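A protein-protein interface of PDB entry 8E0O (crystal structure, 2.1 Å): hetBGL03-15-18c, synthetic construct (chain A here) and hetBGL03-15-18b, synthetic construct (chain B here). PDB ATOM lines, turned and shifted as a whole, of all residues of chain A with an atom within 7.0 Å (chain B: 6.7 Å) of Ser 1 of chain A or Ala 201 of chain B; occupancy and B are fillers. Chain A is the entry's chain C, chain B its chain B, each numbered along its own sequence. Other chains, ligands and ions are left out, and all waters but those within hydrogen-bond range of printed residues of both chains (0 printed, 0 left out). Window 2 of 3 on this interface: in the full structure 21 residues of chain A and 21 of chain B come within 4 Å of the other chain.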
ATOM      1  N   SER A   1      -7.370 -27.460  29.073  1.00  0.00           N
ATOM      2  CA  SER A   1      -8.302 -27.172  30.158  1.00  0.00           C
ATOM      3  C   SER A   1      -9.523 -26.416  29.649  1.00  0.00           C
ATOM      4  O   SER A   1      -9.488 -25.193  29.541  1.00  0.00           O
ATOM      5  CB  SER A   1      -7.614 -26.366  31.260  1.00  0.00           C
ATOM      6  OG  SER A   1      -8.519 -26.081  32.312  1.00  0.00           O
ATOM      7  N   PRO A   2     -10.585 -27.151  29.300  1.00  0.00           N
ATOM      8  CA  PRO A   2     -11.834 -26.489  28.890  1.00  0.00           C
ATOM      9  C   PRO A   2     -12.290 -25.382  29.824  1.00  0.00           C
ATOM     10  O   PRO A   2     -12.826 -24.367  29.358  1.00  0.00           O
ATOM     11  CB  PRO A   2     -12.836 -27.650  28.871  1.00  0.00           C
ATOM     12  CG  PRO A   2     -11.999 -28.923  28.774  1.00  0.00           C
ATOM     13  CD  PRO A   2     -10.546 -28.537  28.804  1.00  0.00           C
ATOM     14  N   ARG A   3     -12.102 -25.553  31.133  1.00  0.00           N
ATOM     15  CA  ARG A   3     -12.485 -24.508  32.076  1.00  0.00           C
ATOM     16  C   ARG A   3     -11.674 -23.236  31.862  1.00  0.00           C
ATOM     17  O   ARG A   3     -12.185 -22.131  32.074  1.00  0.00           O
ATOM     18  CB  ARG A   3     -12.323 -25.015  33.510  1.00  0.00           C
ATOM     19  N   LEU A   4     -10.415 -23.370  31.437  1.00  0.00           N
ATOM     20  CA  LEU A   4      -9.612 -22.191  31.131  1.00  0.00           C
ATOM     21  C   LEU A   4     -10.095 -21.513  29.854  1.00  0.00           C
ATOM     22  O   LEU A   4     -10.154 -20.279  29.783  1.00  0.00           O
ATOM     23  CB  LEU A   4      -8.139 -22.577  31.008  1.00  0.00           C
ATOM     24  CG  LEU A   4      -7.304 -22.569  32.290  1.00  0.00           C
ATOM     25  CD1 LEU A   4      -5.858 -22.931  31.986  1.00  0.00           C
ATOM     26  CD2 LEU A   4      -7.386 -21.217  32.981  1.00  0.00           C
ATOM     27  N   VAL A   5     -10.440 -22.304  28.835  1.00  0.00           N
ATOM     28  CA  VAL A   5     -10.962 -21.738  27.593  1.00  0.00           C
ATOM     29  C   VAL A   5     -12.280 -21.023  27.851  1.00  0.00           C
ATOM     30  O   VAL A   5     -12.513 -19.916  27.349  1.00  0.00           O
ATOM     31  CB  VAL A   5     -11.118 -22.838  26.526  1.00  0.00           C
ATOM     32  CG1 VAL A   5     -11.713 -22.260  25.249  1.00  0.00           C
ATOM     33  CG2 VAL A   5      -9.780 -23.506  26.247  1.00  0.00           C
ATOM     34  N   LEU A   6     -13.164 -21.649  28.634  1.00  0.00           N
ATOM     35  CA  LEU A   6     -14.429 -21.024  29.010  1.00  0.00           C
ATOM     36  C   LEU A   6     -14.211 -19.643  29.612  1.00  0.00           C
ATOM     37  O   LEU A   6     -14.834 -18.660  29.193  1.00  0.00           O
ATOM     38  CB  LEU A   6     -15.169 -21.922  30.003  1.00  0.00           C
ATOM     39  CG  LEU A   6     -16.693 -21.860  30.053  1.00  0.00           C
ATOM     40  CD1 LEU A   6     -17.314 -22.274  28.731  1.00  0.00           C
ATOM     41  CD2 LEU A   6     -17.198 -22.731  31.192  1.00  0.00           C
ATOM     42  N   ARG A   7     -13.314 -19.553  30.596  1.00  0.00           N
ATOM     43  CA  ARG A   7     -13.068 -18.283  31.271  1.00  0.00           C
ATOM     44  C   ARG A   7     -12.445 -17.262  30.325  1.00  0.00           C
ATOM     45  O   ARG A   7     -12.748 -16.065  30.407  1.00  0.00           O
ATOM     46  CB  ARG A   7     -12.174 -18.516  32.489  1.00  0.00           C
ATOM     47  CG  ARG A   7     -11.730 -17.257  33.204  1.00  0.00           C
ATOM     48  CD  ARG A   7     -12.486 -17.079  34.511  1.00  0.00           C
ATOM     49  NE  ARG A   7     -12.222 -15.784  35.127  1.00  0.00           N
ATOM     50  CZ  ARG A   7     -12.653 -14.621  34.655  1.00  0.00           C
ATOM     51  NH1 ARG A   7     -13.390 -14.548  33.558  1.00  0.00           N
ATOM     52  NH2 ARG A   7     -12.338 -13.504  35.302  1.00  0.00           N
ATOM     53  N   ALA A   8     -11.578 -17.715  29.418  1.00  0.00           N
ATOM     54  CA  ALA A   8     -10.963 -16.794  28.467  1.00  0.00           C
ATOM     55  C   ALA A   8     -11.992 -16.243  27.489  1.00  0.00           C
ATOM     56  O   ALA A   8     -11.938 -15.064  27.121  1.00  0.00           O
ATOM     57  CB  ALA A   8      -9.826 -17.491  27.722  1.00  0.00           C
ATOM     58  N   LEU A  49     -16.438 -24.846  21.192  1.00  0.00           N
ATOM     59  CA  LEU A  49     -16.268 -25.352  22.549  1.00  0.00           C
ATOM     60  C   LEU A  49     -17.499 -26.121  23.012  1.00  0.00           C
ATOM     61  O   LEU A  49     -17.378 -27.172  23.652  1.00  0.00           O
ATOM     62  CB  LEU A  49     -15.965 -24.199  23.507  1.00  0.00           C
ATOM     63  CG  LEU A  49     -15.743 -24.568  24.975  1.00  0.00           C
ATOM     64  CD1 LEU A  49     -14.711 -25.680  25.106  1.00  0.00           C
ATOM     65  CD2 LEU A  49     -15.326 -23.347  25.780  1.00  0.00           C
ATOM     66  N   PHE B 150      -2.742 -19.531  34.935  1.00  0.00           N
ATOM     67  CA  PHE B 150      -3.608 -18.977  33.899  1.00  0.00           C
ATOM     68  C   PHE B 150      -4.971 -18.580  34.448  1.00  0.00           C
ATOM     69  O   PHE B 150      -5.572 -17.614  33.963  1.00  0.00           O
ATOM     70  CB  PHE B 150      -3.767 -19.981  32.755  1.00  0.00           C
ATOM     71  CG  PHE B 150      -2.468 -20.375  32.108  1.00  0.00           C
ATOM     72  CD1 PHE B 150      -1.357 -19.550  32.186  1.00  0.00           C
ATOM     73  CD2 PHE B 150      -2.357 -21.577  31.428  1.00  0.00           C
ATOM     74  CE1 PHE B 150      -0.162 -19.914  31.593  1.00  0.00           C
ATOM     75  CE2 PHE B 150      -1.166 -21.946  30.834  1.00  0.00           C
ATOM     76  CZ  PHE B 150      -0.067 -21.113  30.916  1.00  0.00           C
ATOM     77  N   GLU B 196      -4.688 -15.577  23.968  1.00  0.00           N
ATOM     78  CA  GLU B 196      -3.455 -16.352  24.066  1.00  0.00           C
ATOM     79  C   GLU B 196      -3.586 -17.465  25.099  1.00  0.00           C
ATOM     80  O   GLU B 196      -3.127 -18.590  24.873  1.00  0.00           O
ATOM     81  CB  GLU B 196      -2.283 -15.433  24.408  1.00  0.00           C
ATOM     82  CG  GLU B 196      -1.852 -14.527  23.267  1.00  0.00           C
ATOM     83  CD  GLU B 196      -0.825 -13.496  23.697  1.00  0.00           C
ATOM     84  OE1 GLU B 196      -0.438 -13.497  24.884  1.00  0.00           O
ATOM     85  OE2 GLU B 196      -0.402 -12.689  22.845  1.00  0.00           O
ATOM     86  N   ILE B 197      -4.215 -17.169  26.238  1.00  0.00           N
ATOM     87  CA  ILE B 197      -4.426 -18.195  27.253  1.00  0.00           C
ATOM     88  C   ILE B 197      -5.378 -19.268  26.736  1.00  0.00           C
ATOM     89  O   ILE B 197      -5.183 -20.464  26.987  1.00  0.00           O
ATOM     90  CB  ILE B 197      -4.932 -17.555  28.559  1.00  0.00           C
ATOM     91  CG1 ILE B 197      -3.801 -16.781  29.240  1.00  0.00           C
ATOM     92  CG2 ILE B 197      -5.493 -18.610  29.500  1.00  0.00           C
ATOM     93  CD1 ILE B 197      -4.277 -15.652  30.131  1.00  0.00           C
ATOM     94  N   ALA B 198      -6.411 -18.862  25.992  1.00  0.00           N
ATOM     95  CA  ALA B 198      -7.336 -19.835  25.418  1.00  0.00           C
ATOM     96  C   ALA B 198      -6.632 -20.747  24.422  1.00  0.00           C
ATOM     97  O   ALA B 198      -6.915 -21.950  24.362  1.00  0.00           O
ATOM     98  CB  ALA B 198      -8.507 -19.116  24.747  1.00  0.00           C
ATOM     99  N   GLU B 199      -5.710 -20.194  23.630  1.00  0.00           N
ATOM    100  CA  GLU B 199      -4.993 -21.007  22.652  1.00  0.00           C
ATOM    101  C   GLU B 199      -4.010 -21.953  23.332  1.00  0.00           C
ATOM    102  O   GLU B 199      -3.819 -23.088  22.881  1.00  0.00           O
ATOM    103  CB  GLU B 199      -4.268 -20.108  21.650  1.00  0.00           C
ATOM    104  CG  GLU B 199      -5.194 -19.322  20.731  1.00  0.00           C
ATOM    105  CD  GLU B 199      -5.762 -20.161  19.601  1.00  0.00           C
ATOM    106  OE1 GLU B 199      -5.454 -21.370  19.531  1.00  0.00           O
ATOM    107  OE2 GLU B 199      -6.524 -19.609  18.779  1.00  0.00           O
ATOM    108  N   GLN B 200      -3.377 -21.504  24.418  1.00  0.00           N
ATOM    109  CA  GLN B 200      -2.479 -22.381  25.160  1.00  0.00           C
ATOM    110  C   GLN B 200      -3.244 -23.479  25.886  1.00  0.00           C
ATOM    111  O   GLN B 200      -2.729 -24.593  26.041  1.00  0.00           O
ATOM    112  CB  GLN B 200      -1.649 -21.568  26.154  1.00  0.00           C
ATOM    113  N   ALA B 201      -4.470 -23.190  26.332  1.00  0.00           N
ATOM    114  CA  ALA B 201      -5.269 -24.193  27.024  1.00  0.00           C
ATOM    115  C   ALA B 201      -5.802 -25.263  26.080  1.00  0.00           C
ATOM    116  O   ALA B 201      -6.190 -26.341  26.542  1.00  0.00           O
ATOM    117  CB  ALA B 201      -6.429 -23.524  27.763  1.00  0.00           C
ATOM    118  N   ARG B 202      -5.833 -24.991  24.774  1.00  0.00           N
ATOM    119  CA  ARG B 202      -6.252 -26.008  23.817  1.00  0.00           C
ATOM    120  C   ARG B 202      -5.131 -27.000  23.534  1.00  0.00           C
ATOM    121  O   ARG B 202      -5.376 -28.208  23.438  1.00  0.00           O
ATOM    122  CB  ARG B 202      -6.721 -25.348  22.519  1.00  0.00           C
ATOM    123  N   LYS B 203      -3.901 -26.512  23.403  1.00  0.00           N
ATOM    124  CA  LYS B 203      -2.754 -27.376  23.148  1.00  0.00           C
ATOM    125  C   LYS B 203      -2.376 -28.164  24.398  1.00  0.00           C
ATOM    126  O   LYS B 203      -1.274 -28.017  24.927  1.00  0.00           O
ATOM    127  CB  LYS B 203      -1.560 -26.553  22.661  1.00  0.00           C
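Of the 9 printed residues of chain A, 4 touch a printed residue of chain B. Hydrophobic or aromatic side chains of chain A that line the printed part of chain B: Leu 4, Val 5 and Ala 8. Printed residues of chain B that touch a printed residue of chain A: Phe 150, Ala 198 and Ala 201. Hydrophobic or aromatic side chains of chain B that line the printed part of chain A: Phe 150, Ala 198 and Ala 201. Along chain B the printed residues that touch a printed residue of chain A span positions 150 to 201.
N of Leu 4 of chain A lies within hydrogen-bond range of OG of Ser 1 of chain A (3.4 Å).
O of Ala 201 of chain B lies within hydrogen-bond range of N of Ser 1 of chain A (3.0 Å).
Leu 4 of chain A touches Phe 150 of chain B. Leu 4 of chain A touches Ala 201 of chain B (CB to CB, 3.8 Å). O of Ala 198 of chain B touches CG2 of Val 5 of chain A, 3.8 Å away. CB of Ala 201 of chain B touches CG2 of Val 5 of chain A, 3.7 Å away. Ala 198 of chain B touches Ala 8 of chain A (CB to CB, 3.6 Å).
Ser 1 of chain A touches just one residue of chain B: Ala 201 (3.0 Å). Arg 3 of chain A touches none of the printed residues of chain B. Printed residues of chain B within 4 Å of Leu 4 of chain A: Phe 150 and Ala 201. Leu 6 of chain A touches none of the printed residues of chain B. Of the printed residues of chain B, Ala 8 of chain A touches Ala 198. Printed residues of chain A within 4 Å of Phe 150 of chain B: Leu 4 (3.7 Å). Of the printed residues of chain A, Ala 198 of chain B touches Val 5 (3.8 Å) and Ala 8 (3.6 Å). Of chain A, only Ser 1 (3.0 Å), Leu 4 (3.8 Å) and Val 5 (3.7 Å) come within 4 Å of Ala 201 of chain B. The nearest residue of chain A that does not touch Ala 201 of chain B is Pro 2 of chain A (5.3 Å). The nearest printed residue of chain B that does not touch Leu 4 of chain A is Ile 197 of chain B (4.7 Å).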
